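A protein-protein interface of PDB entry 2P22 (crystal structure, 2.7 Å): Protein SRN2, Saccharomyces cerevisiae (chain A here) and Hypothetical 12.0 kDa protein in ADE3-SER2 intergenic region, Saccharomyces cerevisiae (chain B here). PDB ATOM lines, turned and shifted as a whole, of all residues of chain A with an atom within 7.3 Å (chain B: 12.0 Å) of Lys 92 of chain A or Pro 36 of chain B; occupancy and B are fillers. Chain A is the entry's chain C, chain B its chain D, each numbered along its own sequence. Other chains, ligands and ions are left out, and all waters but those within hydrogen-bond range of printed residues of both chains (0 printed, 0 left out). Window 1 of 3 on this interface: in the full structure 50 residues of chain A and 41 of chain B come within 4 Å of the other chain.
The side-chain amide nitrogen (NE2) of Gln 96 of chain A lies close to the side-chain amino group (NZ) of Lys 92 of chain A (2.7 Å).
A ring nitrogen (NE2) of His 89 of chain A is in hydrogen-bond range of the side-chain carboxylate (OD2) of Asp 93 of chain A (3.0 Å).
Leu 38 of chain B touches Leu 88 of chain A (CD1 to O, 3.2 Å).
CA of His 89 of chain A touches CD1 of Leu 38 of chain B, 3.5 Å away.
CB of His 89 of chain A touches NH1 of Arg 42 of chain B, at 3.7 Å.
CE of Lys 92 of chain A touches CB of Leu 35 of chain B, 3.7 Å away.
Lys 92 of chain A touches Pro 36 of chain B.
CG1 of Val 95 of chain A touches CD1 of Leu 35 of chain B (3.6 Å).
CA of Gln 96 of chain A touches CD1 of Leu 35 of chain B, at 3.8 Å.
Of chain B, only Leu 38 comes within 4 Å of Leu 88 of chain A.
Of chain B, only Leu 38 and Arg 42 come within 4 Å of His 89 of chain A.
Lys 92 of chain A touches two residues of chain B.
Val 95 of chain A touches just one residue of chain B: Leu 35.
Gln 96 of chain A touches just one residue of chain B: Leu 35 (3.8 Å).
Of the printed residues of chain A, Leu 35 of chain B touches Lys 92 (3.7 Å), Val 95 (3.6 Å) and Gln 96 (3.8 Å).
Of chain A, only Lys 92 (3.5 Å) comes within 4 Å of Pro 36 of chain B.
Ala 37 of chain B touches none of the printed residues of chain A.
Printed residues of chain A within 4 Å of Leu 38 of chain B: Leu 88 (3.2 Å) and His 89 (3.5 Å).
Of the printed residues of chain A, Arg 42 of chain B touches His 89 (3.7 Å).
The nearest residue of chain B that does not touch Lys 92 of chain A is Leu 38 of chain B (4.1 Å).
The nearest residue of chain A that does not touch Pro 36 of chain B is Leu 88 of chain A (6.6 Å).
Hydrophobic or aromatic side chains of chain B that line the printed part of chain A: Leu 35 and Leu 38.
Hydrophobic or aromatic side chains of chain A within 4 Å of the printed part of chain B: His 89 and Val 95.
Along chain A the printed residues that touch a printed residue of chain B span positions 88 to 96.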
ATOM      1  N   ASP A  87     -27.169  -3.155 -15.568  1.00  0.00           N
ATOM      2  CA  ASP A  87     -27.192  -2.662 -16.938  1.00  0.00           C
ATOM      3  C   ASP A  87     -26.778  -3.788 -17.877  1.00  0.00           C
ATOM      4  O   ASP A  87     -27.452  -4.069 -18.863  1.00  0.00           O
ATOM      5  CB  ASP A  87     -26.238  -1.478 -17.095  1.00  0.00           C
ATOM      6  CG  ASP A  87     -26.492  -0.384 -16.075  1.00  0.00           C
ATOM      7  OD1 ASP A  87     -27.671  -0.032 -15.845  1.00  0.00           O
ATOM      8  OD2 ASP A  87     -25.509   0.134 -15.510  1.00  0.00           O
ATOM      9  N   LEU A  88     -25.665  -4.435 -17.559  1.00  0.00           N
ATOM     10  CA  LEU A  88     -25.175  -5.534 -18.361  1.00  0.00           C
ATOM     11  C   LEU A  88     -26.270  -6.572 -18.539  1.00  0.00           C
ATOM     12  O   LEU A  88     -26.205  -7.399 -19.444  1.00  0.00           O
ATOM     13  CB  LEU A  88     -23.971  -6.165 -17.683  1.00  0.00           C
ATOM     14  CG  LEU A  88     -23.220  -7.186 -18.527  1.00  0.00           C
ATOM     15  CD1 LEU A  88     -22.806  -6.573 -19.852  1.00  0.00           C
ATOM     16  CD2 LEU A  88     -21.998  -7.648 -17.760  1.00  0.00           C
ATOM     17  N   HIS A  89     -27.274  -6.526 -17.668  1.00  0.00           N
ATOM     18  CA  HIS A  89     -28.403  -7.453 -17.741  1.00  0.00           C
ATOM     19  C   HIS A  89     -29.393  -6.951 -18.773  1.00  0.00           C
ATOM     20  O   HIS A  89     -29.863  -7.710 -19.616  1.00  0.00           O
ATOM     21  CB  HIS A  89     -29.118  -7.556 -16.394  1.00  0.00           C
ATOM     22  CG  HIS A  89     -30.477  -8.179 -16.480  1.00  0.00           C
ATOM     23  ND1 HIS A  89     -30.680  -9.471 -16.917  1.00  0.00           N
ATOM     24  CD2 HIS A  89     -31.701  -7.688 -16.178  1.00  0.00           C
ATOM     25  CE1 HIS A  89     -31.972  -9.748 -16.878  1.00  0.00           C
ATOM     26  NE2 HIS A  89     -32.613  -8.683 -16.433  1.00  0.00           N
ATOM     27  N   GLU A  90     -29.714  -5.667 -18.694  1.00  0.00           N
ATOM     28  CA  GLU A  90     -30.648  -5.072 -19.631  1.00  0.00           C
ATOM     29  C   GLU A  90     -30.113  -5.134 -21.056  1.00  0.00           C
ATOM     30  O   GLU A  90     -30.870  -5.387 -21.988  1.00  0.00           O
ATOM     31  CB  GLU A  90     -30.942  -3.634 -19.227  1.00  0.00           C
ATOM     32  CG  GLU A  90     -31.824  -3.535 -17.999  1.00  0.00           C
ATOM     33  CD  GLU A  90     -31.820  -2.147 -17.400  1.00  0.00           C
ATOM     34  OE1 GLU A  90     -32.006  -1.174 -18.162  1.00  0.00           O
ATOM     35  OE2 GLU A  90     -31.633  -2.031 -16.167  1.00  0.00           O
ATOM     36  N   GLN A  91     -28.815  -4.908 -21.232  1.00  0.00           N
ATOM     37  CA  GLN A  91     -28.237  -4.979 -22.566  1.00  0.00           C
ATOM     38  C   GLN A  91     -28.324  -6.423 -23.048  1.00  0.00           C
ATOM     39  O   GLN A  91     -28.774  -6.684 -24.161  1.00  0.00           O
ATOM     40  CB  GLN A  91     -26.774  -4.517 -22.565  1.00  0.00           C
ATOM     41  CG  GLN A  91     -26.584  -2.998 -22.592  1.00  0.00           C
ATOM     42  CD  GLN A  91     -25.167  -2.581 -22.995  1.00  0.00           C
ATOM     43  OE1 GLN A  91     -24.644  -3.029 -24.024  1.00  0.00           O
ATOM     44  NE2 GLN A  91     -24.549  -1.711 -22.194  1.00  0.00           N
ATOM     45  N   LYS A  92     -27.909  -7.362 -22.201  1.00  0.00           N
ATOM     46  CA  LYS A  92     -27.947  -8.778 -22.554  1.00  0.00           C
ATOM     47  C   LYS A  92     -29.370  -9.237 -22.786  1.00  0.00           C
ATOM     48  O   LYS A  92     -29.601 -10.324 -23.312  1.00  0.00           O
ATOM     49  CB  LYS A  92     -27.314  -9.616 -21.452  1.00  0.00           C
ATOM     50  CG  LYS A  92     -27.134 -11.075 -21.797  1.00  0.00           C
ATOM     51  CD  LYS A  92     -28.290 -11.907 -21.326  1.00  0.00           C
ATOM     52  CE  LYS A  92     -27.882 -13.363 -21.190  1.00  0.00           C
ATOM     53  NZ  LYS A  92     -29.052 -14.175 -20.757  1.00  0.00           N
ATOM     54  N   ASP A  93     -30.321  -8.406 -22.382  1.00  0.00           N
ATOM     55  CA  ASP A  93     -31.718  -8.727 -22.580  1.00  0.00           C
ATOM     56  C   ASP A  93     -32.067  -8.513 -24.041  1.00  0.00           C
ATOM     57  O   ASP A  93     -32.710  -9.359 -24.654  1.00  0.00           O
ATOM     58  CB  ASP A  93     -32.617  -7.850 -21.702  1.00  0.00           C
ATOM     59  CG  ASP A  93     -32.903  -8.474 -20.340  1.00  0.00           C
ATOM     60  OD1 ASP A  93     -33.424  -9.617 -20.298  1.00  0.00           O
ATOM     61  OD2 ASP A  93     -32.613  -7.818 -19.311  1.00  0.00           O
ATOM     62  N   LYS A  94     -31.648  -7.385 -24.605  1.00  0.00           N
ATOM     63  CA  LYS A  94     -31.957  -7.131 -26.005  1.00  0.00           C
ATOM     64  C   LYS A  94     -31.260  -8.155 -26.903  1.00  0.00           C
ATOM     65  O   LYS A  94     -31.844  -8.651 -27.866  1.00  0.00           O
ATOM     66  CB  LYS A  94     -31.555  -5.710 -26.414  1.00  0.00           C
ATOM     67  CG  LYS A  94     -31.866  -5.400 -27.886  1.00  0.00           C
ATOM     68  CD  LYS A  94     -31.688  -3.924 -28.218  1.00  0.00           C
ATOM     69  CE  LYS A  94     -32.117  -3.608 -29.648  1.00  0.00           C
ATOM     70  NZ  LYS A  94     -32.030  -2.144 -29.944  1.00  0.00           N
ATOM     71  N   VAL A  95     -30.013  -8.474 -26.579  1.00  0.00           N
ATOM     72  CA  VAL A  95     -29.254  -9.444 -27.349  1.00  0.00           C
ATOM     73  C   VAL A  95     -29.962 -10.789 -27.304  1.00  0.00           C
ATOM     74  O   VAL A  95     -29.909 -11.564 -28.258  1.00  0.00           O
ATOM     75  CB  VAL A  95     -27.837  -9.610 -26.776  1.00  0.00           C
ATOM     76  CG1 VAL A  95     -27.102 -10.734 -27.496  1.00  0.00           C
ATOM     77  CG2 VAL A  95     -27.074  -8.304 -26.905  1.00  0.00           C
ATOM     78  N   GLN A  96     -30.632 -11.063 -26.190  1.00  0.00           N
ATOM     79  CA  GLN A  96     -31.349 -12.323 -26.019  1.00  0.00           C
ATOM     80  C   GLN A  96     -32.574 -12.345 -26.945  1.00  0.00           C
ATOM     81  O   GLN A  96     -33.185 -13.396 -27.167  1.00  0.00           O
ATOM     82  CB  GLN A  96     -31.752 -12.483 -24.541  1.00  0.00           C
ATOM     83  CG  GLN A  96     -32.050 -13.915 -24.092  1.00  0.00           C
ATOM     84  CD  GLN A  96     -31.671 -14.184 -22.628  1.00  0.00           C
ATOM     85  OE1 GLN A  96     -32.082 -13.460 -21.712  1.00  0.00           O
ATOM     86  NE2 GLN A  96     -30.889 -15.241 -22.407  1.00  0.00           N
ATOM     87  N   ALA A  97     -32.902 -11.177 -27.500  1.00  0.00           N
ATOM     88  CA  ALA A  97     -34.036 -11.018 -28.408  1.00  0.00           C
ATOM     89  C   ALA A  97     -33.558 -10.915 -29.858  1.00  0.00           C
ATOM     90  O   ALA A  97     -34.157 -11.487 -30.770  1.00  0.00           O
ATOM     91  CB  ALA A  97     -34.830  -9.783 -28.032  1.00  0.00           C
ATOM     92  N   GLU B  32     -22.268 -20.691 -33.722  1.00  0.00           N
ATOM     93  CA  GLU B  32     -22.758 -20.931 -32.372  1.00  0.00           C
ATOM     94  C   GLU B  32     -22.782 -19.623 -31.586  1.00  0.00           C
ATOM     95  O   GLU B  32     -21.810 -18.871 -31.590  1.00  0.00           O
ATOM     96  CB  GLU B  32     -21.845 -21.941 -31.666  1.00  0.00           C
ATOM     97  CG  GLU B  32     -22.313 -22.366 -30.285  1.00  0.00           C
ATOM     98  CD  GLU B  32     -23.613 -23.136 -30.333  1.00  0.00           C
ATOM     99  OE1 GLU B  32     -23.653 -24.180 -31.017  1.00  0.00           O
ATOM    100  OE2 GLU B  32     -24.591 -22.699 -29.689  1.00  0.00           O
ATOM    101  N   PHE B  33     -23.895 -19.350 -30.919  1.00  0.00           N
ATOM    102  CA  PHE B  33     -24.016 -18.137 -30.126  1.00  0.00           C
ATOM    103  C   PHE B  33     -24.265 -18.474 -28.670  1.00  0.00           C
ATOM    104  O   PHE B  33     -25.166 -19.248 -28.348  1.00  0.00           O
ATOM    105  CB  PHE B  33     -25.154 -17.276 -30.651  1.00  0.00           C
ATOM    106  CG  PHE B  33     -24.865 -16.651 -31.969  1.00  0.00           C
ATOM    107  CD1 PHE B  33     -25.669 -16.916 -33.068  1.00  0.00           C
ATOM    108  CD2 PHE B  33     -23.783 -15.796 -32.116  1.00  0.00           C
ATOM    109  CE1 PHE B  33     -25.398 -16.332 -34.296  1.00  0.00           C
ATOM    110  CE2 PHE B  33     -23.502 -15.208 -33.338  1.00  0.00           C
ATOM    111  CZ  PHE B  33     -24.311 -15.476 -34.432  1.00  0.00           C
ATOM    112  N   LYS B  34     -23.470 -17.886 -27.787  1.00  0.00           N
ATOM    113  CA  LYS B  34     -23.613 -18.144 -26.364  1.00  0.00           C
ATOM    114  C   LYS B  34     -23.587 -16.839 -25.566  1.00  0.00           C
ATOM    115  O   LYS B  34     -22.610 -16.095 -25.603  1.00  0.00           O
ATOM    116  CB  LYS B  34     -22.474 -19.047 -25.888  1.00  0.00           C
ATOM    117  CG  LYS B  34     -22.110 -20.187 -26.831  1.00  0.00           C
ATOM    118  CD  LYS B  34     -20.815 -20.844 -26.375  1.00  0.00           C
ATOM    119  CE  LYS B  34     -20.258 -21.810 -27.412  1.00  0.00           C
ATOM    120  NZ  LYS B  34     -18.956 -22.399 -26.965  1.00  0.00           N
ATOM    121  N   LEU B  35     -24.660 -16.556 -24.842  1.00  0.00           N
ATOM    122  CA  LEU B  35     -24.689 -15.351 -24.040  1.00  0.00           C
ATOM    123  C   LEU B  35     -24.348 -15.720 -22.597  1.00  0.00           C
ATOM    124  O   LEU B  35     -24.993 -16.578 -21.993  1.00  0.00           O
ATOM    125  CB  LEU B  35     -26.063 -14.697 -24.125  1.00  0.00           C
ATOM    126  CG  LEU B  35     -26.573 -14.487 -25.555  1.00  0.00           C
ATOM    127  CD1 LEU B  35     -27.835 -13.637 -25.506  1.00  0.00           C
ATOM    128  CD2 LEU B  35     -25.515 -13.820 -26.417  1.00  0.00           C
ATOM    129  N   PRO B  36     -23.326 -15.063 -22.025  1.00  0.00           N
ATOM    130  CA  PRO B  36     -22.872 -15.311 -20.655  1.00  0.00           C
ATOM    131  C   PRO B  36     -23.933 -15.194 -19.578  1.00  0.00           C
ATOM    132  O   PRO B  36     -24.903 -14.449 -19.713  1.00  0.00           O
ATOM    133  CB  PRO B  36     -21.757 -14.288 -20.478  1.00  0.00           C
ATOM    134  CG  PRO B  36     -22.226 -13.151 -21.317  1.00  0.00           C
ATOM    135  CD  PRO B  36     -22.676 -13.857 -22.567  1.00  0.00           C
ATOM    136  N   ALA B  37     -23.728 -15.946 -18.503  1.00  0.00           N
ATOM    137  CA  ALA B  37     -24.652 -15.934 -17.383  1.00  0.00           C
ATOM    138  C   ALA B  37     -24.336 -14.761 -16.470  1.00  0.00           C
ATOM    139  O   ALA B  37     -23.172 -14.467 -16.184  1.00  0.00           O
ATOM    140  CB  ALA B  37     -24.557 -17.225 -16.618  1.00  0.00           C
ATOM    141  N   LEU B  38     -25.387 -14.091 -16.018  1.00  0.00           N
ATOM    142  CA  LEU B  38     -25.218 -12.949 -15.147  1.00  0.00           C
ATOM    143  C   LEU B  38     -25.868 -13.137 -13.780  1.00  0.00           C
ATOM    144  O   LEU B  38     -25.317 -12.712 -12.763  1.00  0.00           O
ATOM    145  CB  LEU B  38     -25.788 -11.700 -15.812  1.00  0.00           C
ATOM    146  CG  LEU B  38     -25.452 -11.445 -17.276  1.00  0.00           C
ATOM    147  CD1 LEU B  38     -26.011 -10.069 -17.629  1.00  0.00           C
ATOM    148  CD2 LEU B  38     -23.962 -11.491 -17.539  1.00  0.00           C
ATOM    149  N   GLN B  39     -27.027 -13.785 -13.743  1.00  0.00           N
ATOM    150  CA  GLN B  39     -27.731 -13.967 -12.476  1.00  0.00           C
ATOM    151  C   GLN B  39     -26.911 -14.577 -11.338  1.00  0.00           C
ATOM    152  O   GLN B  39     -26.904 -14.041 -10.236  1.00  0.00           O
ATOM    153  CB  GLN B  39     -29.004 -14.788 -12.678  1.00  0.00           C
ATOM    154  CG  GLN B  39     -30.010 -14.596 -11.556  1.00  0.00           C
ATOM    155  CD  GLN B  39     -30.389 -13.131 -11.373  1.00  0.00           C
ATOM    156  OE1 GLN B  39     -30.947 -12.499 -12.275  1.00  0.00           O
ATOM    157  NE2 GLN B  39     -30.077 -12.583 -10.205  1.00  0.00           N
ATOM    158  N   PRO B  40     -26.210 -15.696 -11.586  1.00  0.00           N
ATOM    159  CA  PRO B  40     -25.409 -16.324 -10.532  1.00  0.00           C
ATOM    160  C   PRO B  40     -24.429 -15.338  -9.930  1.00  0.00           C
ATOM    161  O   PRO B  40     -24.396 -15.150  -8.711  1.00  0.00           O
ATOM    162  CB  PRO B  40     -24.706 -17.460 -11.258  1.00  0.00           C
ATOM    163  CG  PRO B  40     -25.679 -17.791 -12.369  1.00  0.00           C
ATOM    164  CD  PRO B  40     -26.046 -16.415 -12.855  1.00  0.00           C
ATOM    165  N   THR B  41     -23.630 -14.701 -10.781  1.00  0.00           N
ATOM    166  CA  THR B  41     -22.652 -13.721 -10.311  1.00  0.00           C
ATOM    167  C   THR B  41     -23.358 -12.580  -9.600  1.00  0.00           C
ATOM    168  O   THR B  41     -22.872 -12.066  -8.591  1.00  0.00           O
ATOM    169  CB  THR B  41     -21.831 -13.139 -11.470  1.00  0.00           C
ATOM    170  OG1 THR B  41     -21.065 -14.187 -12.080  1.00  0.00           O
ATOM    171  CG2 THR B  41     -20.899 -12.058 -10.959  1.00  0.00           C
ATOM    172  N   ARG B  42     -24.507 -12.188 -10.137  1.00  0.00           N
ATOM    173  CA  ARG B  42     -25.301 -11.123  -9.541  1.00  0.00           C
ATOM    174  C   ARG B  42     -25.639 -11.485  -8.095  1.00  0.00           C
ATOM    175  O   ARG B  42     -25.567 -10.641  -7.202  1.00  0.00           O
ATOM    176  CB  ARG B  42     -26.588 -10.925 -10.338  1.00  0.00           C
ATOM    177  CG  ARG B  42     -26.490  -9.864 -11.406  1.00  0.00           C
ATOM    178  CD  ARG B  42     -26.885  -8.523 -10.837  1.00  0.00           C
ATOM    179  NE  ARG B  42     -28.330  -8.421 -10.660  1.00  0.00           N
ATOM    180  CZ  ARG B  42     -29.204  -8.479 -11.659  1.00  0.00           C
ATOM    181  NH1 ARG B  42     -28.773  -8.638 -12.901  1.00  0.00           N
ATOM    182  NH2 ARG B  42     -30.505  -8.370 -11.421  1.00  0.00           N
